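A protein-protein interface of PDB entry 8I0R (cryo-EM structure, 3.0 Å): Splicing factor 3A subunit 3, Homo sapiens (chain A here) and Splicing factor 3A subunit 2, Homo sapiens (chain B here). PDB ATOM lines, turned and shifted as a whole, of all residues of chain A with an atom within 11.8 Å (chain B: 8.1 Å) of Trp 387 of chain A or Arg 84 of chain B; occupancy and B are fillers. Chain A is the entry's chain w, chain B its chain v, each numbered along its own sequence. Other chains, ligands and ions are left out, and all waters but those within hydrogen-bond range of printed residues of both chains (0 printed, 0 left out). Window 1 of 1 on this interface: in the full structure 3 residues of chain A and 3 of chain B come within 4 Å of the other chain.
The side-chain carboxylate of Asp 388 of chain A is in salt-bridge range of the guanidinium group of Arg 84 of chain B (3.2 Å).
OD2 of Asp 388 of chain A is in salt-bridge range of NZ of Lys 390 of chain A (3.7 Å).
CD of Arg 84 of chain B touches CH2 of Trp 387 of chain A, 3.9 Å away. NH1 of Arg 85 of chain B touches CZ3 of Trp 387 of chain A, 3.6 Å away. NZ of Lys 91 of chain B touches O of Asp 388 of chain A, at 3.6 Å. Lys 390 of chain A touches Arg 84 of chain B.
Trp 387 of chain A touches two residues of chain B. Arg 84 of chain B touches just these residues of chain A: Trp 387 (3.9 Å), Asp 388 (3.2 Å) and Lys 390 (3.2 Å). No residue of chain B comes within 4 Å of Gly 386 of chain A. No residue of chain A comes within 4 Å of Thr 80 of chain B. No residue of chain A comes within 4 Å of Asn 81 of chain B. No residue of chain A comes within 4 Å of Ala 83 of chain B. Arg 85 of chain B touches just one residue of chain A: Trp 387. No residue of chain A comes within 4 Å of Ala 87 of chain B. Lys 88 of chain B touches none of the printed residues of chain A. Of the printed residues of chain B, Asp 388 of chain A touches Arg 84 (3.2 Å) and Lys 91 (3.6 Å). Of the printed residues of chain A, Lys 91 of chain B touches Asp 388 (3.6 Å). Printed residues of chain B within 4 Å of Lys 390 of chain A: Arg 84. Ile 392 of chain A touches none of the printed residues of chain B. The nearest residue of chain A that does not touch Arg 84 of chain B is Pro 391 of chain A (6.4 Å). The nearest printed residue of chain B that does not touch Lys 390 of chain A is Ala 87 of chain B (5.0 Å).
Hydrophobic or aromatic side chains of chain A within 4 Å of the printed part of chain B: Trp 387. Along chain A the printed residues that touch a printed residue of chain B span positions 387 to 390. Among the printed residues, Asp or Glu carboxylates within 4 Å of a Lys or Arg side-chain nitrogen of the other chain: Asp 388 of chain A with Arg 84 of chain B.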
ATOM      1  N   LYS A 381     -10.826   6.745  26.274  1.00  0.00           N
ATOM      2  CA  LYS A 381     -10.842   6.739  24.818  1.00  0.00           C
ATOM      3  C   LYS A 381     -11.923   5.807  24.272  1.00  0.00           C
ATOM      4  O   LYS A 381     -12.971   6.254  23.803  1.00  0.00           O
ATOM      5  CB  LYS A 381      -9.471   6.336  24.264  1.00  0.00           C
ATOM      6  CG  LYS A 381      -8.515   7.501  24.077  1.00  0.00           C
ATOM      7  CD  LYS A 381      -7.341   7.131  23.175  1.00  0.00           C
ATOM      8  CE  LYS A 381      -7.795   6.762  21.767  1.00  0.00           C
ATOM      9  NZ  LYS A 381      -6.692   6.163  20.967  1.00  0.00           N
ATOM     10  N   LEU A 383     -12.155   3.686  21.654  1.00  0.00           N
ATOM     11  CA  LEU A 383     -12.572   3.636  20.267  1.00  0.00           C
ATOM     12  C   LEU A 383     -12.856   2.195  19.856  1.00  0.00           C
ATOM     13  O   LEU A 383     -12.380   1.255  20.497  1.00  0.00           O
ATOM     14  CB  LEU A 383     -11.496   4.230  19.369  1.00  0.00           C
ATOM     15  CG  LEU A 383     -11.489   5.759  19.360  1.00  0.00           C
ATOM     16  CD1 LEU A 383     -10.337   6.327  18.544  1.00  0.00           C
ATOM     17  CD2 LEU A 383     -12.823   6.300  18.867  1.00  0.00           C
ATOM     18  N   PRO A 384     -13.658   2.000  18.815  1.00  0.00           N
ATOM     19  CA  PRO A 384     -13.795   0.661  18.237  1.00  0.00           C
ATOM     20  C   PRO A 384     -12.434   0.107  17.845  1.00  0.00           C
ATOM     21  O   PRO A 384     -11.516   0.852  17.496  1.00  0.00           O
ATOM     22  CB  PRO A 384     -14.681   0.891  17.010  1.00  0.00           C
ATOM     23  CG  PRO A 384     -15.343   2.199  17.223  1.00  0.00           C
ATOM     24  CD  PRO A 384     -14.666   2.945  18.316  1.00  0.00           C
ATOM     25  N   LEU A 385     -12.303  -1.213  17.908  1.00  0.00           N
ATOM     26  CA  LEU A 385     -11.050  -1.850  17.532  1.00  0.00           C
ATOM     27  C   LEU A 385     -11.023  -2.141  16.039  1.00  0.00           C
ATOM     28  O   LEU A 385     -11.888  -2.842  15.509  1.00  0.00           O
ATOM     29  CB  LEU A 385     -10.839  -3.133  18.332  1.00  0.00           C
ATOM     30  CG  LEU A 385     -10.009  -2.945  19.600  1.00  0.00           C
ATOM     31  CD1 LEU A 385      -8.553  -2.835  19.222  1.00  0.00           C
ATOM     32  CD2 LEU A 385     -10.436  -1.711  20.378  1.00  0.00           C
ATOM     33  N   GLY A 386     -10.009  -1.607  15.365  1.00  0.00           N
ATOM     34  CA  GLY A 386      -9.904  -1.732  13.930  1.00  0.00           C
ATOM     35  C   GLY A 386      -9.450  -3.105  13.498  1.00  0.00           C
ATOM     36  O   GLY A 386      -9.113  -3.978  14.299  1.00  0.00           O
ATOM     37  N   TRP A 387      -9.467  -3.298  12.181  1.00  0.00           N
ATOM     38  CA  TRP A 387      -9.017  -4.540  11.572  1.00  0.00           C
ATOM     39  C   TRP A 387      -7.557  -4.840  11.873  1.00  0.00           C
ATOM     40  O   TRP A 387      -7.158  -6.006  11.844  1.00  0.00           O
ATOM     41  CB  TRP A 387      -9.236  -4.446  10.066  1.00  0.00           C
ATOM     42  CG  TRP A 387      -8.526  -3.276   9.474  1.00  0.00           C
ATOM     43  CD1 TRP A 387      -9.030  -2.027   9.265  1.00  0.00           C
ATOM     44  CD2 TRP A 387      -7.173  -3.244   9.015  1.00  0.00           C
ATOM     45  NE1 TRP A 387      -8.074  -1.218   8.702  1.00  0.00           N
ATOM     46  CE2 TRP A 387      -6.924  -1.944   8.538  1.00  0.00           C
ATOM     47  CE3 TRP A 387      -6.150  -4.193   8.957  1.00  0.00           C
ATOM     48  CZ2 TRP A 387      -5.699  -1.569   8.019  1.00  0.00           C
ATOM     49  CZ3 TRP A 387      -4.941  -3.820   8.443  1.00  0.00           C
ATOM     50  CH2 TRP A 387      -4.720  -2.519   7.979  1.00  0.00           C
ATOM     51  N   ASP A 388      -6.758  -3.817  12.146  1.00  0.00           N
ATOM     52  CA  ASP A 388      -5.371  -3.974  12.550  1.00  0.00           C
ATOM     53  C   ASP A 388      -5.208  -3.971  14.061  1.00  0.00           C
ATOM     54  O   ASP A 388      -4.138  -3.601  14.556  1.00  0.00           O
ATOM     55  CB  ASP A 388      -4.509  -2.874  11.923  1.00  0.00           C
ATOM     56  CG  ASP A 388      -5.121  -1.499  12.065  1.00  0.00           C
ATOM     57  OD1 ASP A 388      -6.362  -1.407  12.170  1.00  0.00           O
ATOM     58  OD2 ASP A 388      -4.365  -0.504  12.070  1.00  0.00           O
ATOM     59  N   GLY A 389      -6.247  -4.357  14.804  1.00  0.00           N
ATOM     60  CA  GLY A 389      -6.201  -4.319  16.249  1.00  0.00           C
ATOM     61  C   GLY A 389      -5.993  -2.945  16.844  1.00  0.00           C
ATOM     62  O   GLY A 389      -5.675  -2.847  18.034  1.00  0.00           O
ATOM     63  N   LYS A 390      -6.121  -1.876  16.042  1.00  0.00           N
ATOM     64  CA  LYS A 390      -5.930  -0.506  16.467  1.00  0.00           C
ATOM     65  C   LYS A 390      -7.265   0.215  16.571  1.00  0.00           C
ATOM     66  O   LYS A 390      -8.271  -0.243  16.027  1.00  0.00           O
ATOM     67  CB  LYS A 390      -5.021   0.245  15.489  1.00  0.00           C
ATOM     68  CG  LYS A 390      -3.528   0.110  15.771  1.00  0.00           C
ATOM     69  CD  LYS A 390      -2.715   0.379  14.505  1.00  0.00           C
ATOM     70  CE  LYS A 390      -1.423  -0.425  14.476  1.00  0.00           C
ATOM     71  NZ  LYS A 390      -0.828  -0.422  13.131  1.00  0.00           N
ATOM     72  N   PRO A 391      -7.312   1.321  17.306  1.00  0.00           N
ATOM     73  CA  PRO A 391      -8.529   2.139  17.329  1.00  0.00           C
ATOM     74  C   PRO A 391      -8.654   2.978  16.062  1.00  0.00           C
ATOM     75  O   PRO A 391      -7.704   3.638  15.637  1.00  0.00           O
ATOM     76  CB  PRO A 391      -8.337   3.011  18.574  1.00  0.00           C
ATOM     77  CG  PRO A 391      -7.383   2.232  19.427  1.00  0.00           C
ATOM     78  CD  PRO A 391      -6.441   1.610  18.456  1.00  0.00           C
ATOM     79  N   ILE A 392      -9.835   2.928  15.452  1.00  0.00           N
ATOM     80  CA  ILE A 392     -10.150   3.641  14.213  1.00  0.00           C
ATOM     81  C   ILE A 392     -10.219   5.145  14.465  1.00  0.00           C
ATOM     82  O   ILE A 392     -10.376   5.570  15.615  1.00  0.00           O
ATOM     83  CB  ILE A 392     -11.472   3.133  13.617  1.00  0.00           C
ATOM     84  CG1 ILE A 392     -12.625   3.415  14.575  1.00  0.00           C
ATOM     85  CG2 ILE A 392     -11.397   1.647  13.322  1.00  0.00           C
ATOM     86  CD1 ILE A 392     -13.972   3.233  13.936  1.00  0.00           C
ATOM     87  N   PRO A 393     -10.121   5.979  13.429  1.00  0.00           N
ATOM     88  CA  PRO A 393     -10.136   7.433  13.633  1.00  0.00           C
ATOM     89  C   PRO A 393     -11.409   7.937  14.296  1.00  0.00           C
ATOM     90  O   PRO A 393     -12.496   7.394  14.098  1.00  0.00           O
ATOM     91  CB  PRO A 393     -10.006   7.986  12.214  1.00  0.00           C
ATOM     92  CG  PRO A 393      -9.365   6.924  11.448  1.00  0.00           C
ATOM     93  CD  PRO A 393      -9.812   5.628  12.035  1.00  0.00           C
ATOM     94  N   TYR A 394     -11.257   9.004  15.083  1.00  0.00           N
ATOM     95  CA  TYR A 394     -12.404   9.646  15.712  1.00  0.00           C
ATOM     96  C   TYR A 394     -13.417  10.131  14.685  1.00  0.00           C
ATOM     97  O   TYR A 394     -14.625  10.052  14.928  1.00  0.00           O
ATOM     98  CB  TYR A 394     -11.937  10.810  16.578  1.00  0.00           C
ATOM     99  CG  TYR A 394     -13.007  11.404  17.458  1.00  0.00           C
ATOM    100  CD1 TYR A 394     -13.522  12.669  17.202  1.00  0.00           C
ATOM    101  CD2 TYR A 394     -13.493  10.707  18.554  1.00  0.00           C
ATOM    102  CE1 TYR A 394     -14.495  13.220  18.010  1.00  0.00           C
ATOM    103  CE2 TYR A 394     -14.469  11.249  19.368  1.00  0.00           C
ATOM    104  CZ  TYR A 394     -14.967  12.508  19.090  1.00  0.00           C
ATOM    105  OH  TYR A 394     -15.940  13.051  19.898  1.00  0.00           O
ATOM    106  N   TRP A 395     -12.958  10.624  13.534  1.00  0.00           N
ATOM    107  CA  TRP A 395     -13.906  11.082  12.521  1.00  0.00           C
ATOM    108  C   TRP A 395     -14.644   9.915  11.877  1.00  0.00           C
ATOM    109  O   TRP A 395     -15.843  10.019  11.610  1.00  0.00           O
ATOM    110  CB  TRP A 395     -13.195  11.915  11.454  1.00  0.00           C
ATOM    111  CG  TRP A 395     -12.129  11.167  10.748  1.00  0.00           C
ATOM    112  CD1 TRP A 395     -10.808  11.138  11.067  1.00  0.00           C
ATOM    113  CD2 TRP A 395     -12.290  10.316   9.613  1.00  0.00           C
ATOM    114  NE1 TRP A 395     -10.130  10.331  10.192  1.00  0.00           N
ATOM    115  CE2 TRP A 395     -11.019   9.806   9.294  1.00  0.00           C
ATOM    116  CE3 TRP A 395     -13.383   9.935   8.834  1.00  0.00           C
ATOM    117  CZ2 TRP A 395     -10.813   8.934   8.234  1.00  0.00           C
ATOM    118  CZ3 TRP A 395     -13.177   9.069   7.786  1.00  0.00           C
ATOM    119  CH2 TRP A 395     -11.903   8.580   7.493  1.00  0.00           C
ATOM    120  N   LEU A 396     -13.953   8.806  11.608  1.00  0.00           N
ATOM    121  CA  LEU A 396     -14.641   7.616  11.127  1.00  0.00           C
ATOM    122  C   LEU A 396     -15.675   7.149  12.138  1.00  0.00           C
ATOM    123  O   LEU A 396     -16.785   6.746  11.770  1.00  0.00           O
ATOM    124  CB  LEU A 396     -13.635   6.498  10.861  1.00  0.00           C
ATOM    125  CG  LEU A 396     -13.566   5.819   9.492  1.00  0.00           C
ATOM    126  CD1 LEU A 396     -12.121   5.572   9.117  1.00  0.00           C
ATOM    127  CD2 LEU A 396     -14.345   4.523   9.473  1.00  0.00           C
ATOM    128  N   HIS A 400     -19.692   6.758  11.472  1.00  0.00           N
ATOM    129  CA  HIS A 400     -20.420   5.515  11.669  1.00  0.00           C
ATOM    130  C   HIS A 400     -21.430   5.585  12.800  1.00  0.00           C
ATOM    131  O   HIS A 400     -22.167   4.617  13.004  1.00  0.00           O
ATOM    132  CB  HIS A 400     -19.438   4.372  11.923  1.00  0.00           C
ATOM    133  CG  HIS A 400     -19.340   3.404  10.788  1.00  0.00           C
ATOM    134  ND1 HIS A 400     -19.953   2.171  10.811  1.00  0.00           N
ATOM    135  CD2 HIS A 400     -18.739   3.502   9.579  1.00  0.00           C
ATOM    136  CE1 HIS A 400     -19.714   1.541   9.676  1.00  0.00           C
ATOM    137  NE2 HIS A 400     -18.980   2.327   8.910  1.00  0.00           N
ATOM    138  N   LEU A 402     -21.295   5.438  16.117  1.00  0.00           N
ATOM    139  CA  LEU A 402     -21.197   4.357  17.085  1.00  0.00           C
ATOM    140  C   LEU A 402     -21.512   4.806  18.502  1.00  0.00           C
ATOM    141  O   LEU A 402     -22.073   4.019  19.269  1.00  0.00           O
ATOM    142  CB  LEU A 402     -19.808   3.743  17.014  1.00  0.00           C
ATOM    143  CG  LEU A 402     -19.665   2.871  15.773  1.00  0.00           C
ATOM    144  CD1 LEU A 402     -18.221   2.783  15.338  1.00  0.00           C
ATOM    145  CD2 LEU A 402     -20.230   1.497  16.057  1.00  0.00           C
ATOM    146  N   TYR B  45       1.333  -5.924  -4.427  1.00  0.00           N
ATOM    147  CA  TYR B  45       0.098  -5.219  -4.132  1.00  0.00           C
ATOM    148  C   TYR B  45      -0.545  -4.470  -5.280  1.00  0.00           C
ATOM    149  O   TYR B  45      -1.381  -3.605  -5.037  1.00  0.00           O
ATOM    150  CB  TYR B  45       0.367  -4.230  -3.018  1.00  0.00           C
ATOM    151  CG  TYR B  45       0.406  -4.899  -1.699  1.00  0.00           C
ATOM    152  CD1 TYR B  45      -0.515  -5.874  -1.387  1.00  0.00           C
ATOM    153  CD2 TYR B  45       1.380  -4.588  -0.777  1.00  0.00           C
ATOM    154  CE1 TYR B  45      -0.485  -6.503  -0.186  1.00  0.00           C
ATOM    155  CE2 TYR B  45       1.423  -5.211   0.423  1.00  0.00           C
ATOM    156  CZ  TYR B  45       0.486  -6.170   0.717  1.00  0.00           C
ATOM    157  OH  TYR B  45       0.515  -6.807   1.927  1.00  0.00           O
ATOM    158  N   LEU B  58      -3.939  -3.281  -1.735  1.00  0.00           N
ATOM    159  CA  LEU B  58      -3.813  -3.109  -0.296  1.00  0.00           C
ATOM    160  C   LEU B  58      -4.636  -1.932   0.188  1.00  0.00           C
ATOM    161  O   LEU B  58      -5.559  -2.105   0.985  1.00  0.00           O
ATOM    162  CB  LEU B  58      -2.349  -2.925   0.076  1.00  0.00           C
ATOM    163  CG  LEU B  58      -2.044  -2.407   1.473  1.00  0.00           C
ATOM    164  CD1 LEU B  58      -1.913  -3.559   2.426  1.00  0.00           C
ATOM    165  CD2 LEU B  58      -0.768  -1.609   1.446  1.00  0.00           C
ATOM    166  N   LYS B  76       1.820   8.656   2.090  1.00  0.00           N
ATOM    167  CA  LYS B  76       1.467   8.357   3.472  1.00  0.00           C
ATOM    168  C   LYS B  76       0.525   7.171   3.573  1.00  0.00           C
ATOM    169  O   LYS B  76       0.787   6.229   4.318  1.00  0.00           O
ATOM    170  CB  LYS B  76       0.835   9.577   4.141  1.00  0.00           C
ATOM    171  CG  LYS B  76      -0.173   9.208   5.216  1.00  0.00           C
ATOM    172  CD  LYS B  76      -0.128  10.156   6.399  1.00  0.00           C
ATOM    173  CE  LYS B  76      -0.898   9.592   7.589  1.00  0.00           C
ATOM    174  NZ  LYS B  76      -0.742  10.444   8.798  1.00  0.00           N
ATOM    175  N   LYS B  77      -0.564   7.206   2.816  1.00  0.00           N
ATOM    176  CA  LYS B  77      -1.555   6.140   2.858  1.00  0.00           C
ATOM    177  C   LYS B  77      -0.913   4.778   2.644  1.00  0.00           C
ATOM    178  O   LYS B  77      -1.062   3.866   3.469  1.00  0.00           O
ATOM    179  CB  LYS B  77      -2.607   6.423   1.794  1.00  0.00           C
ATOM    180  CG  LYS B  77      -3.891   5.663   1.890  1.00  0.00           C
ATOM    181  CD  LYS B  77      -5.001   6.535   1.366  1.00  0.00           C
ATOM    182  CE  LYS B  77      -6.351   5.914   1.594  1.00  0.00           C
ATOM    183  NZ  LYS B  77      -6.559   4.747   0.713  1.00  0.00           N
ATOM    184  N   HIS B  78      -0.173   4.630   1.554  1.00  0.00           N
ATOM    185  CA  HIS B  78       0.396   3.333   1.238  1.00  0.00           C
ATOM    186  C   HIS B  78       1.399   2.905   2.289  1.00  0.00           C
ATOM    187  O   HIS B  78       1.421   1.741   2.694  1.00  0.00           O
ATOM    188  CB  HIS B  78       1.061   3.366  -0.123  1.00  0.00           C
ATOM    189  CG  HIS B  78       1.425   2.019  -0.633  1.00  0.00           C
ATOM    190  ND1 HIS B  78       0.497   1.141  -1.142  1.00  0.00           N
ATOM    191  CD2 HIS B  78       2.616   1.390  -0.709  1.00  0.00           C
ATOM    192  CE1 HIS B  78       1.102   0.031  -1.511  1.00  0.00           C
ATOM    193  NE2 HIS B  78       2.389   0.154  -1.258  1.00  0.00           N
ATOM    194  N   GLN B  79       2.236   3.832   2.745  1.00  0.00           N
ATOM    195  CA  GLN B  79       3.281   3.478   3.694  1.00  0.00           C
ATOM    196  C   GLN B  79       2.699   3.045   5.026  1.00  0.00           C
ATOM    197  O   GLN B  79       3.133   2.043   5.597  1.00  0.00           O
ATOM    198  CB  GLN B  79       4.231   4.649   3.884  1.00  0.00           C
ATOM    199  CG  GLN B  79       4.689   5.247   2.600  1.00  0.00           C
ATOM    200  CD  GLN B  79       5.869   4.527   2.023  1.00  0.00           C
ATOM    201  OE1 GLN B  79       5.759   3.392   1.574  1.00  0.00           O
ATOM    202  NE2 GLN B  79       7.012   5.182   2.029  1.00  0.00           N
ATOM    203  N   THR B  80       1.724   3.782   5.548  1.00  0.00           N
ATOM    204  CA  THR B  80       1.161   3.384   6.827  1.00  0.00           C
ATOM    205  C   THR B  80       0.395   2.078   6.714  1.00  0.00           C
ATOM    206  O   THR B  80       0.450   1.252   7.627  1.00  0.00           O
ATOM    207  CB  THR B  80       0.278   4.479   7.394  1.00  0.00           C
ATOM    208  OG1 THR B  80      -0.968   4.496   6.697  1.00  0.00           O
ATOM    209  CG2 THR B  80       0.968   5.807   7.278  1.00  0.00           C
ATOM    210  N   ASN B  81      -0.332   1.859   5.619  1.00  0.00           N
ATOM    211  CA  ASN B  81      -0.983   0.563   5.476  1.00  0.00           C
ATOM    212  C   ASN B  81       0.044  -0.558   5.388  1.00  0.00           C
ATOM    213  O   ASN B  81      -0.166  -1.648   5.932  1.00  0.00           O
ATOM    214  CB  ASN B  81      -1.892   0.567   4.258  1.00  0.00           C
ATOM    215  CG  ASN B  81      -2.976   1.599   4.363  1.00  0.00           C
ATOM    216  OD1 ASN B  81      -3.590   1.756   5.411  1.00  0.00           O
ATOM    217  ND2 ASN B  81      -3.211   2.323   3.284  1.00  0.00           N
ATOM    218  N   LEU B  82       1.179  -0.295   4.744  1.00  0.00           N
ATOM    219  CA  LEU B  82       2.233  -1.297   4.647  1.00  0.00           C
ATOM    220  C   LEU B  82       2.825  -1.593   6.014  1.00  0.00           C
ATOM    221  O   LEU B  82       3.108  -2.748   6.350  1.00  0.00           O
ATOM    222  CB  LEU B  82       3.308  -0.806   3.686  1.00  0.00           C
ATOM    223  CG  LEU B  82       3.961  -1.839   2.791  1.00  0.00           C
ATOM    224  CD1 LEU B  82       3.006  -2.955   2.571  1.00  0.00           C
ATOM    225  CD2 LEU B  82       4.313  -1.198   1.490  1.00  0.00           C
ATOM    226  N   ALA B  83       2.999  -0.556   6.827  1.00  0.00           N
ATOM    227  CA  ALA B  83       3.507  -0.747   8.178  1.00  0.00           C
ATOM    228  C   ALA B  83       2.526  -1.552   9.023  1.00  0.00           C
ATOM    229  O   ALA B  83       2.920  -2.466   9.754  1.00  0.00           O
ATOM    230  CB  ALA B  83       3.797   0.606   8.815  1.00  0.00           C
ATOM    231  N   ARG B  84       1.241  -1.218   8.945  1.00  0.00           N
ATOM    232  CA  ARG B  84       0.246  -2.016   9.648  1.00  0.00           C
ATOM    233  C   ARG B  84       0.301  -3.471   9.223  1.00  0.00           C
ATOM    234  O   ARG B  84       0.182  -4.365  10.059  1.00  0.00           O
ATOM    235  CB  ARG B  84      -1.158  -1.471   9.417  1.00  0.00           C
ATOM    236  CG  ARG B  84      -1.415  -0.130  10.034  1.00  0.00           C
ATOM    237  CD  ARG B  84      -2.704   0.429   9.505  1.00  0.00           C
ATOM    238  NE  ARG B  84      -2.677   1.884   9.379  1.00  0.00           N
ATOM    239  CZ  ARG B  84      -2.773   2.719  10.404  1.00  0.00           C
ATOM    240  NH1 ARG B  84      -2.753   4.023  10.192  1.00  0.00           N
ATOM    241  NH2 ARG B  84      -2.887   2.253  11.638  1.00  0.00           N
ATOM    242  N   ARG B  85       0.439  -3.744   7.929  1.00  0.00           N
ATOM    243  CA  ARG B  85       0.427  -5.146   7.536  1.00  0.00           C
ATOM    244  C   ARG B  85       1.697  -5.856   7.974  1.00  0.00           C
ATOM    245  O   ARG B  85       1.667  -7.044   8.317  1.00  0.00           O
ATOM    246  CB  ARG B  85       0.218  -5.302   6.042  1.00  0.00           C
ATOM    247  CG  ARG B  85       0.112  -6.757   5.652  1.00  0.00           C
ATOM    248  CD  ARG B  85      -0.946  -6.974   4.604  1.00  0.00           C
ATOM    249  NE  ARG B  85      -2.155  -7.531   5.193  1.00  0.00           N
ATOM    250  CZ  ARG B  85      -3.080  -6.814   5.820  1.00  0.00           C
ATOM    251  NH1 ARG B  85      -2.941  -5.503   5.929  1.00  0.00           N
ATOM    252  NH2 ARG B  85      -4.146  -7.408   6.333  1.00  0.00           N
ATOM    253  N   ALA B  86       2.826  -5.152   7.971  1.00  0.00           N
ATOM    254  CA  ALA B  86       4.044  -5.748   8.509  1.00  0.00           C
ATOM    255  C   ALA B  86       3.864  -6.113   9.974  1.00  0.00           C
ATOM    256  O   ALA B  86       4.212  -7.223  10.401  1.00  0.00           O
ATOM    257  CB  ALA B  86       5.216  -4.790   8.336  1.00  0.00           C
ATOM    258  N   ALA B  87       3.317  -5.183  10.759  1.00  0.00           N
ATOM    259  CA  ALA B  87       2.977  -5.485  12.145  1.00  0.00           C
ATOM    260  C   ALA B  87       2.077  -6.708  12.237  1.00  0.00           C
ATOM    261  O   ALA B  87       2.423  -7.680  12.908  1.00  0.00           O
ATOM    262  CB  ALA B  87       2.312  -4.276  12.797  1.00  0.00           C
ATOM    263  N   LYS B  88       0.935  -6.678  11.548  1.00  0.00           N
ATOM    264  CA  LYS B  88      -0.014  -7.785  11.593  1.00  0.00           C
ATOM    265  C   LYS B  88       0.659  -9.118  11.299  1.00  0.00           C
ATOM    266  O   LYS B  88       0.357 -10.129  11.943  1.00  0.00           O
ATOM    267  CB  LYS B  88      -1.151  -7.541  10.605  1.00  0.00           C
ATOM    268  CG  LYS B  88      -2.207  -8.627  10.620  1.00  0.00           C
ATOM    269  CD  LYS B  88      -2.861  -8.738  11.983  1.00  0.00           C
ATOM    270  CE  LYS B  88      -4.046  -9.683  11.952  1.00  0.00           C
ATOM    271  NZ  LYS B  88      -4.976  -9.417  10.817  1.00  0.00           N
ATOM    272  N   GLU B  89       1.592  -9.143  10.350  1.00  0.00           N
ATOM    273  CA  GLU B  89       2.293 -10.392  10.084  1.00  0.00           C
ATOM    274  C   GLU B  89       3.194 -10.764  11.256  1.00  0.00           C
ATOM    275  O   GLU B  89       3.316 -11.944  11.603  1.00  0.00           O
ATOM    276  CB  GLU B  89       3.098 -10.291   8.790  1.00  0.00           C
ATOM    277  CG  GLU B  89       3.693 -11.616   8.321  1.00  0.00           C
ATOM    278  CD  GLU B  89       4.885 -12.051   9.147  1.00  0.00           C
ATOM    279  OE1 GLU B  89       4.992 -13.256   9.463  1.00  0.00           O
ATOM    280  OE2 GLU B  89       5.699 -11.175   9.501  1.00  0.00           O
ATOM    281  N   ALA B  90       3.840  -9.772  11.875  1.00  0.00           N
ATOM    282  CA  ALA B  90       4.650 -10.069  13.056  1.00  0.00           C
ATOM    283  C   ALA B  90       3.799 -10.702  14.148  1.00  0.00           C
ATOM    284  O   ALA B  90       4.175 -11.726  14.728  1.00  0.00           O
ATOM    285  CB  ALA B  90       5.328  -8.801  13.570  1.00  0.00           C
ATOM    286  N   LYS B  91       2.653 -10.087  14.445  1.00  0.00           N
ATOM    287  CA  LYS B  91       1.632 -10.726  15.271  1.00  0.00           C
ATOM    288  C   LYS B  91       1.373 -12.156  14.819  1.00  0.00           C
ATOM    289  O   LYS B  91       1.193 -13.058  15.645  1.00  0.00           O
ATOM    290  CB  LYS B  91       0.334  -9.923  15.210  1.00  0.00           C
ATOM    291  CG  LYS B  91       0.495  -8.438  15.440  1.00  0.00           C
ATOM    292  CD  LYS B  91      -0.792  -7.833  15.973  1.00  0.00           C
ATOM    293  CE  LYS B  91      -0.708  -6.321  16.050  1.00  0.00           C
ATOM    294  NZ  LYS B  91      -1.992  -5.746  16.527  1.00  0.00           N
